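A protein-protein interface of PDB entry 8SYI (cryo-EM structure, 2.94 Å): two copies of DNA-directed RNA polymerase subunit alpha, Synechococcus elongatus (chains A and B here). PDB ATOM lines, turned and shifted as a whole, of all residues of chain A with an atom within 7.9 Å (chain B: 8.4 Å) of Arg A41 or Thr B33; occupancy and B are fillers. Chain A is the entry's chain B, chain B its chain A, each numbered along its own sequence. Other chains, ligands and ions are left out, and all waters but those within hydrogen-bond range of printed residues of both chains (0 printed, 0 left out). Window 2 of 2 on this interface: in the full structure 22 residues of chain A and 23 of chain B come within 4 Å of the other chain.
Of chain B, only Gly B30, Thr B33 and Thr B34 come within 4 Å of Arg A41.
Ser A45 touches none of the printed residues of chain B.
Of the printed residues of chain B, Asn A46 touches Gln B31 (3.4 Å).
Of the printed residues of chain A, Gly B30 touches Arg A41.
Of the printed residues of chain A, Gln B31 touches Asn A46.
Of the printed residues of chain A, Thr B33 touches Arg A41.
Val B179 touches none of the printed residues of chain A.
The nearest printed residue of chain B that does not touch Asn A46 is Ala B28 (4.6 Å).
Positions printed for both chains: 35, 36, 37, 38, 39, 40 and 177.
Of the 4 pairs that touch across the chains among the printed residues, none has its exchanged pair printed and touching as well.
Thr B33 touches Arg A41 (CB to NH2, 3.9 Å).
NE of Arg A41 touches CG2 of Thr B34, 3.4 Å away.
Of the 18 printed residues of chain A, 2 touch a printed residue of chain B.
Printed residues of chain A that touch a printed residue of chain B: Arg A41 and Asn A46.
Among the printed residues, 4 pairs touch across the chains.
Among the printed residues, no Asp or Glu carboxylate lies within 4 Å of a Lys or Arg side-chain nitrogen of the other chain.
The backbone NH (N) of Gly B30 is in hydrogen-bond range of the side-chain carboxylate (OD1) of Asp B191, 3.4 Å away.
The backbone carbonyl oxygen of Gly B30 is in hydrogen-bond range of the guanidinium group of Arg A41, 3.3 Å away.
NE2 of Gln B31 is in hydrogen-bond range of OD1 of Asn A46 (3.4 Å).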
ATOM      1  N   VAL A  35      -0.753  21.931   8.945  1.00  0.00           N
ATOM      2  CA  VAL A  35       0.677  21.725   9.148  1.00  0.00           C
ATOM      3  C   VAL A  35       1.471  22.918   8.634  1.00  0.00           C
ATOM      4  O   VAL A  35       2.390  23.402   9.307  1.00  0.00           O
ATOM      5  CB  VAL A  35       1.124  20.412   8.480  1.00  0.00           C
ATOM      6  CG1 VAL A  35       2.625  20.247   8.584  1.00  0.00           C
ATOM      7  CG2 VAL A  35       0.424  19.236   9.121  1.00  0.00           C
ATOM      8  N   GLY A  36       1.122  23.425   7.450  1.00  0.00           N
ATOM      9  CA  GLY A  36       1.880  24.521   6.875  1.00  0.00           C
ATOM     10  C   GLY A  36       1.816  25.786   7.706  1.00  0.00           C
ATOM     11  O   GLY A  36       2.839  26.417   7.969  1.00  0.00           O
ATOM     12  N   ASN A  37       0.615  26.173   8.140  1.00  0.00           N
ATOM     13  CA  ASN A  37       0.491  27.407   8.907  1.00  0.00           C
ATOM     14  C   ASN A  37       1.104  27.268  10.294  1.00  0.00           C
ATOM     15  O   ASN A  37       1.759  28.200  10.785  1.00  0.00           O
ATOM     16  CB  ASN A  37      -0.971  27.826   9.005  1.00  0.00           C
ATOM     17  CG  ASN A  37      -1.131  29.313   9.204  1.00  0.00           C
ATOM     18  OD1 ASN A  37      -0.980  30.095   8.268  1.00  0.00           O
ATOM     19  ND2 ASN A  37      -1.429  29.716  10.429  1.00  0.00           N
ATOM     20  N   ALA A  38       0.912  26.115  10.945  1.00  0.00           N
ATOM     21  CA  ALA A  38       1.527  25.914  12.249  1.00  0.00           C
ATOM     22  C   ALA A  38       3.046  25.936  12.161  1.00  0.00           C
ATOM     23  O   ALA A  38       3.708  26.449  13.068  1.00  0.00           O
ATOM     24  CB  ALA A  38       1.045  24.600  12.859  1.00  0.00           C
ATOM     25  N   LEU A  39       3.620  25.389  11.085  1.00  0.00           N
ATOM     26  CA  LEU A  39       5.067  25.452  10.915  1.00  0.00           C
ATOM     27  C   LEU A  39       5.530  26.870  10.605  1.00  0.00           C
ATOM     28  O   LEU A  39       6.555  27.317  11.126  1.00  0.00           O
ATOM     29  CB  LEU A  39       5.508  24.499   9.807  1.00  0.00           C
ATOM     30  CG  LEU A  39       5.701  23.027  10.164  1.00  0.00           C
ATOM     31  CD1 LEU A  39       6.100  22.252   8.930  1.00  0.00           C
ATOM     32  CD2 LEU A  39       6.739  22.873  11.254  1.00  0.00           C
ATOM     33  N   ARG A  40       4.795  27.583   9.750  1.00  0.00           N
ATOM     34  CA  ARG A  40       5.187  28.933   9.356  1.00  0.00           C
ATOM     35  C   ARG A  40       5.251  29.866  10.554  1.00  0.00           C
ATOM     36  O   ARG A  40       6.234  30.597  10.736  1.00  0.00           O
ATOM     37  CB  ARG A  40       4.202  29.472   8.323  1.00  0.00           C
ATOM     38  CG  ARG A  40       4.783  30.478   7.363  1.00  0.00           C
ATOM     39  CD  ARG A  40       3.701  31.084   6.497  1.00  0.00           C
ATOM     40  NE  ARG A  40       3.452  32.479   6.838  1.00  0.00           N
ATOM     41  CZ  ARG A  40       4.024  33.509   6.231  1.00  0.00           C
ATOM     42  NH1 ARG A  40       4.875  33.338   5.235  1.00  0.00           N
ATOM     43  NH2 ARG A  40       3.732  34.742   6.633  1.00  0.00           N
ATOM     44  N   ARG A  41       4.206  29.859  11.385  1.00  0.00           N
ATOM     45  CA  ARG A  41       4.154  30.785  12.513  1.00  0.00           C
ATOM     46  C   ARG A  41       5.316  30.556  13.472  1.00  0.00           C
ATOM     47  O   ARG A  41       5.986  31.506  13.899  1.00  0.00           O
ATOM     48  CB  ARG A  41       2.819  30.638  13.237  1.00  0.00           C
ATOM     49  CG  ARG A  41       1.628  31.115  12.436  1.00  0.00           C
ATOM     50  CD  ARG A  41       0.364  31.108  13.273  1.00  0.00           C
ATOM     51  NE  ARG A  41       0.448  32.046  14.383  1.00  0.00           N
ATOM     52  CZ  ARG A  41      -0.249  33.169  14.469  1.00  0.00           C
ATOM     53  NH1 ARG A  41      -1.111  33.519  13.532  1.00  0.00           N
ATOM     54  NH2 ARG A  41      -0.077  33.958  15.524  1.00  0.00           N
ATOM     55  N   VAL A  42       5.585  29.292  13.802  1.00  0.00           N
ATOM     56  CA  VAL A  42       6.643  28.970  14.751  1.00  0.00           C
ATOM     57  C   VAL A  42       8.013  29.262  14.155  1.00  0.00           C
ATOM     58  O   VAL A  42       8.897  29.795  14.835  1.00  0.00           O
ATOM     59  CB  VAL A  42       6.520  27.505  15.202  1.00  0.00           C
ATOM     60  CG1 VAL A  42       7.810  27.035  15.830  1.00  0.00           C
ATOM     61  CG2 VAL A  42       5.377  27.355  16.179  1.00  0.00           C
ATOM     62  N   LEU A  43       8.216  28.924  12.880  1.00  0.00           N
ATOM     63  CA  LEU A  43       9.504  29.176  12.246  1.00  0.00           C
ATOM     64  C   LEU A  43       9.813  30.661  12.204  1.00  0.00           C
ATOM     65  O   LEU A  43      10.949  31.075  12.464  1.00  0.00           O
ATOM     66  CB  LEU A  43       9.518  28.596  10.833  1.00  0.00           C
ATOM     67  CG  LEU A  43       9.882  27.123  10.664  1.00  0.00           C
ATOM     68  CD1 LEU A  43       9.771  26.716   9.213  1.00  0.00           C
ATOM     69  CD2 LEU A  43      11.276  26.870  11.177  1.00  0.00           C
ATOM     70  N   LEU A  44       8.817  31.485  11.887  1.00  0.00           N
ATOM     71  CA  LEU A  44       9.075  32.908  11.731  1.00  0.00           C
ATOM     72  C   LEU A  44       9.095  33.670  13.048  1.00  0.00           C
ATOM     73  O   LEU A  44       9.714  34.734  13.111  1.00  0.00           O
ATOM     74  CB  LEU A  44       8.035  33.531  10.803  1.00  0.00           C
ATOM     75  CG  LEU A  44       8.309  33.396   9.308  1.00  0.00           C
ATOM     76  CD1 LEU A  44       7.126  33.900   8.517  1.00  0.00           C
ATOM     77  CD2 LEU A  44       9.571  34.142   8.930  1.00  0.00           C
ATOM     78  N   SER A  45       8.451  33.169  14.105  1.00  0.00           N
ATOM     79  CA  SER A  45       8.256  33.996  15.290  1.00  0.00           C
ATOM     80  C   SER A  45       8.807  33.443  16.597  1.00  0.00           C
ATOM     81  O   SER A  45       8.832  34.193  17.578  1.00  0.00           O
ATOM     82  CB  SER A  45       6.764  34.289  15.489  1.00  0.00           C
ATOM     83  OG  SER A  45       6.580  35.374  16.381  1.00  0.00           O
ATOM     84  N   ASN A  46       9.248  32.184  16.667  1.00  0.00           N
ATOM     85  CA  ASN A  46       9.527  31.581  17.967  1.00  0.00           C
ATOM     86  C   ASN A  46      10.881  30.878  18.038  1.00  0.00           C
ATOM     87  O   ASN A  46      11.077  30.029  18.912  1.00  0.00           O
ATOM     88  CB  ASN A  46       8.415  30.601  18.346  1.00  0.00           C
ATOM     89  CG  ASN A  46       7.245  31.282  19.014  1.00  0.00           C
ATOM     90  OD1 ASN A  46       6.091  31.061  18.650  1.00  0.00           O
ATOM     91  ND2 ASN A  46       7.534  32.121  19.997  1.00  0.00           N
ATOM     92  N   LEU A  47      11.821  31.210  17.160  1.00  0.00           N
ATOM     93  CA  LEU A  47      13.162  30.648  17.210  1.00  0.00           C
ATOM     94  C   LEU A  47      14.147  31.687  17.731  1.00  0.00           C
ATOM     95  O   LEU A  47      14.030  32.878  17.433  1.00  0.00           O
ATOM     96  CB  LEU A  47      13.611  30.154  15.832  1.00  0.00           C
ATOM     97  CG  LEU A  47      12.951  28.890  15.272  1.00  0.00           C
ATOM     98  CD1 LEU A  47      13.836  28.254  14.217  1.00  0.00           C
ATOM     99  CD2 LEU A  47      12.645  27.903  16.379  1.00  0.00           C
ATOM    100  N   VAL A 175       9.462  32.126   4.629  1.00  0.00           N
ATOM    101  CA  VAL A 175       8.862  30.796   4.584  1.00  0.00           C
ATOM    102  C   VAL A 175       7.674  30.839   3.634  1.00  0.00           C
ATOM    103  O   VAL A 175       6.849  31.753   3.712  1.00  0.00           O
ATOM    104  CB  VAL A 175       8.411  30.310   5.976  1.00  0.00           C
ATOM    105  CG1 VAL A 175       7.759  28.949   5.873  1.00  0.00           C
ATOM    106  CG2 VAL A 175       9.582  30.254   6.938  1.00  0.00           C
ATOM    107  N   TYR A 177       4.650  28.104   1.614  1.00  0.00           N
ATOM    108  CA  TYR A 177       4.102  26.759   1.543  1.00  0.00           C
ATOM    109  C   TYR A 177       2.973  26.717   0.525  1.00  0.00           C
ATOM    110  O   TYR A 177       2.330  27.727   0.237  1.00  0.00           O
ATOM    111  CB  TYR A 177       3.630  26.262   2.918  1.00  0.00           C
ATOM    112  CG  TYR A 177       2.312  26.816   3.412  1.00  0.00           C
ATOM    113  CD1 TYR A 177       2.260  27.996   4.133  1.00  0.00           C
ATOM    114  CD2 TYR A 177       1.122  26.136   3.185  1.00  0.00           C
ATOM    115  CE1 TYR A 177       1.063  28.495   4.593  1.00  0.00           C
ATOM    116  CE2 TYR A 177      -0.080  26.630   3.640  1.00  0.00           C
ATOM    117  CZ  TYR A 177      -0.102  27.806   4.344  1.00  0.00           C
ATOM    118  OH  TYR A 177      -1.297  28.302   4.802  1.00  0.00           O
ATOM    119  N   ALA A 212      11.499  23.672  14.983  1.00  0.00           N
ATOM    120  CA  ALA A 212      10.086  24.034  14.994  1.00  0.00           C
ATOM    121  C   ALA A 212       9.216  22.848  15.385  1.00  0.00           C
ATOM    122  O   ALA A 212       8.280  22.992  16.176  1.00  0.00           O
ATOM    123  CB  ALA A 212       9.671  24.578  13.629  1.00  0.00           C
ATOM    124  N   CYS A 215       9.531  22.219  19.100  1.00  0.00           N
ATOM    125  CA  CYS A 215       8.773  23.177  19.895  1.00  0.00           C
ATOM    126  C   CYS A 215       7.268  22.970  19.765  1.00  0.00           C
ATOM    127  O   CYS A 215       6.524  23.281  20.700  1.00  0.00           O
ATOM    128  CB  CYS A 215       9.150  24.605  19.499  1.00  0.00           C
ATOM    129  SG  CYS A 215       7.755  25.683  19.122  1.00  0.00           S
ATOM    130  N   LEU A 216       6.803  22.456  18.624  1.00  0.00           N
ATOM    131  CA  LEU A 216       5.372  22.219  18.451  1.00  0.00           C
ATOM    132  C   LEU A 216       4.904  20.969  19.183  1.00  0.00           C
ATOM    133  O   LEU A 216       3.774  20.937  19.681  1.00  0.00           O
ATOM    134  CB  LEU A 216       5.030  22.113  16.969  1.00  0.00           C
ATOM    135  CG  LEU A 216       4.691  23.415  16.252  1.00  0.00           C
ATOM    136  CD1 LEU A 216       4.915  23.256  14.769  1.00  0.00           C
ATOM    137  CD2 LEU A 216       3.266  23.824  16.531  1.00  0.00           C
ATOM    138  N   LEU B  27       0.698  30.849  27.885  1.00  0.00           N
ATOM    139  CA  LEU B  27       1.346  30.709  26.594  1.00  0.00           C
ATOM    140  C   LEU B  27       2.310  31.885  26.406  1.00  0.00           C
ATOM    141  O   LEU B  27       2.540  32.658  27.338  1.00  0.00           O
ATOM    142  CB  LEU B  27       0.272  30.604  25.509  1.00  0.00           C
ATOM    143  CG  LEU B  27      -0.514  29.293  25.560  1.00  0.00           C
ATOM    144  CD1 LEU B  27      -1.695  29.331  24.620  1.00  0.00           C
ATOM    145  CD2 LEU B  27       0.386  28.121  25.236  1.00  0.00           C
ATOM    146  N   ALA B  28       2.888  32.036  25.203  1.00  0.00           N
ATOM    147  CA  ALA B  28       3.961  33.022  25.005  1.00  0.00           C
ATOM    148  C   ALA B  28       3.689  33.910  23.785  1.00  0.00           C
ATOM    149  O   ALA B  28       4.201  33.663  22.694  1.00  0.00           O
ATOM    150  CB  ALA B  28       5.314  32.326  24.883  1.00  0.00           C
ATOM    151  N   ARG B  29       2.897  34.964  23.995  1.00  0.00           N
ATOM    152  CA  ARG B  29       2.777  36.092  23.071  1.00  0.00           C
ATOM    153  C   ARG B  29       2.572  35.704  21.612  1.00  0.00           C
ATOM    154  O   ARG B  29       3.486  35.841  20.794  1.00  0.00           O
ATOM    155  CB  ARG B  29       3.995  37.010  23.184  1.00  0.00           C
ATOM    156  CG  ARG B  29       3.769  38.405  22.590  1.00  0.00           C
ATOM    157  CD  ARG B  29       2.942  39.319  23.496  1.00  0.00           C
ATOM    158  NE  ARG B  29       1.542  38.920  23.585  1.00  0.00           N
ATOM    159  CZ  ARG B  29       0.645  39.491  24.376  1.00  0.00           C
ATOM    160  NH1 ARG B  29       0.950  40.532  25.134  1.00  0.00           N
ATOM    161  NH2 ARG B  29      -0.593  39.006  24.408  1.00  0.00           N
ATOM    162  N   GLY B  30       1.394  35.192  21.279  1.00  0.00           N
ATOM    163  CA  GLY B  30       1.082  34.828  19.918  1.00  0.00           C
ATOM    164  C   GLY B  30       0.980  33.343  19.678  1.00  0.00           C
ATOM    165  O   GLY B  30       0.553  32.935  18.593  1.00  0.00           O
ATOM    166  N   GLN B  31       1.361  32.527  20.655  1.00  0.00           N
ATOM    167  CA  GLN B  31       1.189  31.086  20.600  1.00  0.00           C
ATOM    168  C   GLN B  31      -0.230  30.662  20.922  1.00  0.00           C
ATOM    169  O   GLN B  31      -0.564  29.488  20.747  1.00  0.00           O
ATOM    170  CB  GLN B  31       2.161  30.407  21.565  1.00  0.00           C
ATOM    171  CG  GLN B  31       3.597  30.440  21.098  1.00  0.00           C
ATOM    172  CD  GLN B  31       4.491  29.537  21.909  1.00  0.00           C
ATOM    173  OE1 GLN B  31       4.243  29.297  23.088  1.00  0.00           O
ATOM    174  NE2 GLN B  31       5.542  29.032  21.284  1.00  0.00           N
ATOM    175  N   GLY B  32      -1.068  31.577  21.398  1.00  0.00           N
ATOM    176  CA  GLY B  32      -2.462  31.268  21.633  1.00  0.00           C
ATOM    177  C   GLY B  32      -3.206  30.982  20.349  1.00  0.00           C
ATOM    178  O   GLY B  32      -3.964  30.016  20.267  1.00  0.00           O
ATOM    179  N   THR B  33      -2.971  31.808  19.329  1.00  0.00           N
ATOM    180  CA  THR B  33      -3.709  31.676  18.077  1.00  0.00           C
ATOM    181  C   THR B  33      -3.328  30.408  17.325  1.00  0.00           C
ATOM    182  O   THR B  33      -4.202  29.721  16.785  1.00  0.00           O
ATOM    183  CB  THR B  33      -3.482  32.906  17.203  1.00  0.00           C
ATOM    184  OG1 THR B  33      -3.649  34.088  17.991  1.00  0.00           O
ATOM    185  CG2 THR B  33      -4.471  32.933  16.062  1.00  0.00           C
ATOM    186  N   THR B  34      -2.036  30.075  17.272  1.00  0.00           N
ATOM    187  CA  THR B  34      -1.621  28.870  16.559  1.00  0.00           C
ATOM    188  C   THR B  34      -2.197  27.620  17.213  1.00  0.00           C
ATOM    189  O   THR B  34      -2.765  26.755  16.534  1.00  0.00           O
ATOM    190  CB  THR B  34      -0.095  28.784  16.486  1.00  0.00           C
ATOM    191  OG1 THR B  34       0.355  27.623  17.191  1.00  0.00           O
ATOM    192  CG2 THR B  34       0.548  30.011  17.084  1.00  0.00           C
ATOM    193  N   VAL B  35      -2.086  27.526  18.539  1.00  0.00           N
ATOM    194  CA  VAL B  35      -2.625  26.377  19.260  1.00  0.00           C
ATOM    195  C   VAL B  35      -4.135  26.295  19.079  1.00  0.00           C
ATOM    196  O   VAL B  35      -4.685  25.229  18.774  1.00  0.00           O
ATOM    197  CB  VAL B  35      -2.241  26.451  20.747  1.00  0.00           C
ATOM    198  CG1 VAL B  35      -2.957  25.376  21.534  1.00  0.00           C
ATOM    199  CG2 VAL B  35      -0.748  26.318  20.910  1.00  0.00           C
ATOM    200  N   GLY B  36      -4.826  27.425  19.244  1.00  0.00           N
ATOM    201  CA  GLY B  36      -6.272  27.413  19.147  1.00  0.00           C
ATOM    202  C   GLY B  36      -6.771  27.020  17.774  1.00  0.00           C
ATOM    203  O   GLY B  36      -7.715  26.240  17.650  1.00  0.00           O
ATOM    204  N   ASN B  37      -6.148  27.550  16.719  1.00  0.00           N
ATOM    205  CA  ASN B  37      -6.631  27.244  15.380  1.00  0.00           C
ATOM    206  C   ASN B  37      -6.267  25.827  14.965  1.00  0.00           C
ATOM    207  O   ASN B  37      -7.048  25.167  14.272  1.00  0.00           O
ATOM    208  CB  ASN B  37      -6.100  28.257  14.376  1.00  0.00           C
ATOM    209  CG  ASN B  37      -7.016  28.420  13.187  1.00  0.00           C
ATOM    210  OD1 ASN B  37      -8.172  28.809  13.331  1.00  0.00           O
ATOM    211  ND2 ASN B  37      -6.507  28.118  12.006  1.00  0.00           N
ATOM    212  N   ALA B  38      -5.101  25.327  15.383  1.00  0.00           N
ATOM    213  CA  ALA B  38      -4.789  23.929  15.123  1.00  0.00           C
ATOM    214  C   ALA B  38      -5.807  23.012  15.788  1.00  0.00           C
ATOM    215  O   ALA B  38      -6.302  22.062  15.165  1.00  0.00           O
ATOM    216  CB  ALA B  38      -3.378  23.610  15.606  1.00  0.00           C
ATOM    217  N   LEU B  39      -6.155  23.299  17.047  1.00  0.00           N
ATOM    218  CA  LEU B  39      -7.149  22.490  17.745  1.00  0.00           C
ATOM    219  C   LEU B  39      -8.515  22.582  17.077  1.00  0.00           C
ATOM    220  O   LEU B  39      -9.195  21.566  16.899  1.00  0.00           O
ATOM    221  CB  LEU B  39      -7.241  22.922  19.204  1.00  0.00           C
ATOM    222  CG  LEU B  39      -6.165  22.380  20.135  1.00  0.00           C
ATOM    223  CD1 LEU B  39      -6.315  22.977  21.511  1.00  0.00           C
ATOM    224  CD2 LEU B  39      -6.236  20.875  20.198  1.00  0.00           C
ATOM    225  N   ARG B  40      -8.936  23.790  16.702  1.00  0.00           N
ATOM    226  CA  ARG B  40     -10.245  23.957  16.082  1.00  0.00           C
ATOM    227  C   ARG B  40     -10.318  23.248  14.739  1.00  0.00           C
ATOM    228  O   ARG B  40     -11.364  22.706  14.372  1.00  0.00           O
ATOM    229  CB  ARG B  40     -10.568  25.439  15.910  1.00  0.00           C
ATOM    230  CG  ARG B  40     -11.995  25.677  15.478  1.00  0.00           C
ATOM    231  CD  ARG B  40     -12.325  27.136  15.290  1.00  0.00           C
ATOM    232  NE  ARG B  40     -13.569  27.291  14.549  1.00  0.00           N
ATOM    233  CZ  ARG B  40     -13.658  27.284  13.228  1.00  0.00           C
ATOM    234  NH1 ARG B  40     -12.588  27.163  12.464  1.00  0.00           N
ATOM    235  NH2 ARG B  40     -14.853  27.401  12.658  1.00  0.00           N
ATOM    236  N   TYR B 177     -12.846  29.684  20.385  1.00  0.00           N
ATOM    237  CA  TYR B 177     -11.687  29.967  21.218  1.00  0.00           C
ATOM    238  C   TYR B 177     -11.416  31.462  21.219  1.00  0.00           C
ATOM    239  O   TYR B 177     -11.804  32.187  20.302  1.00  0.00           O
ATOM    240  CB  TYR B 177     -10.446  29.192  20.752  1.00  0.00           C
ATOM    241  CG  TYR B 177      -9.764  29.757  19.529  1.00  0.00           C
ATOM    242  CD1 TYR B 177     -10.200  29.430  18.257  1.00  0.00           C
ATOM    243  CD2 TYR B 177      -8.673  30.607  19.648  1.00  0.00           C
ATOM    244  CE1 TYR B 177      -9.581  29.944  17.143  1.00  0.00           C
ATOM    245  CE2 TYR B 177      -8.051  31.126  18.536  1.00  0.00           C
ATOM    246  CZ  TYR B 177      -8.508  30.788  17.289  1.00  0.00           C
ATOM    247  OH  TYR B 177      -7.893  31.296  16.176  1.00  0.00           O
ATOM    248  N   SER B 178     -10.743  31.914  22.273  1.00  0.00           N
ATOM    249  CA  SER B 178     -10.394  33.324  22.404  1.00  0.00           C
ATOM    250  C   SER B 178      -9.167  33.452  23.288  1.00  0.00           C
ATOM    251  O   SER B 178      -9.053  32.753  24.298  1.00  0.00           O
ATOM    252  CB  SER B 178     -11.551  34.129  22.991  1.00  0.00           C
ATOM    253  OG  SER B 178     -11.317  34.417  24.356  1.00  0.00           O
ATOM    254  N   VAL B 179      -8.265  34.354  22.921  1.00  0.00           N
ATOM    255  CA  VAL B 179      -7.010  34.550  23.636  1.00  0.00           C
ATOM    256  C   VAL B 179      -7.067  35.893  24.351  1.00  0.00           C
ATOM    257  O   VAL B 179      -7.371  36.923  23.740  1.00  0.00           O
ATOM    258  CB  VAL B 179      -5.806  34.467  22.686  1.00  0.00           C
ATOM    259  CG1 VAL B 179      -6.230  34.799  21.270  1.00  0.00           C
ATOM    260  CG2 VAL B 179      -4.688  35.378  23.149  1.00  0.00           C
ATOM    261  N   ASP B 191       0.102  35.172  27.667  1.00  0.00           N
ATOM    262  CA  ASP B 191      -1.183  34.896  27.038  1.00  0.00           C
ATOM    263  C   ASP B 191      -1.976  33.861  27.829  1.00  0.00           C
ATOM    264  O   ASP B 191      -1.426  33.119  28.647  1.00  0.00           O
ATOM    265  CB  ASP B 191      -0.997  34.396  25.603  1.00  0.00           C
ATOM    266  CG  ASP B 191      -1.104  35.504  24.582  1.00  0.00           C
ATOM    267  OD1 ASP B 191      -1.272  35.196  23.385  1.00  0.00           O
ATOM    268  OD2 ASP B 191      -1.016  36.685  24.978  1.00  0.00           O
ATOM    269  N   ARG B 192      -3.284  33.816  27.569  1.00  0.00           N
ATOM    270  CA  ARG B 192      -4.161  32.799  28.143  1.00  0.00           C
ATOM    271  C   ARG B 192      -5.226  32.441  27.119  1.00  0.00           C
ATOM    272  O   ARG B 192      -5.879  33.331  26.573  1.00  0.00           O
ATOM    273  CB  ARG B 192      -4.810  33.295  29.437  1.00  0.00           C
ATOM    274  CG  ARG B 192      -5.956  32.425  29.923  1.00  0.00           C
ATOM    275  CD  ARG B 192      -6.792  33.134  30.969  1.00  0.00           C
ATOM    276  NE  ARG B 192      -5.997  34.053  31.772  1.00  0.00           N
ATOM    277  CZ  ARG B 192      -6.458  34.729  32.814  1.00  0.00           C
ATOM    278  NH1 ARG B 192      -7.714  34.612  33.211  1.00  0.00           N
ATOM    279  NH2 ARG B 192      -5.639  35.542  33.475  1.00  0.00           N
ATOM    280  N   LEU B 193      -5.416  31.151  26.860  1.00  0.00           N
ATOM    281  CA  LEU B 193      -6.379  30.695  25.867  1.00  0.00           C
ATOM    282  C   LEU B 193      -7.605  30.109  26.555  1.00  0.00           C
ATOM    283  O   LEU B 193      -7.484  29.398  27.555  1.00  0.00           O
ATOM    284  CB  LEU B 193      -5.740  29.652  24.947  1.00  0.00           C
ATOM    285  CG  LEU B 193      -6.592  28.980  23.873  1.00  0.00           C
ATOM    286  CD1 LEU B 193      -6.846  29.917  22.718  1.00  0.00           C
ATOM    287  CD2 LEU B 193      -5.910  27.721  23.394  1.00  0.00           C
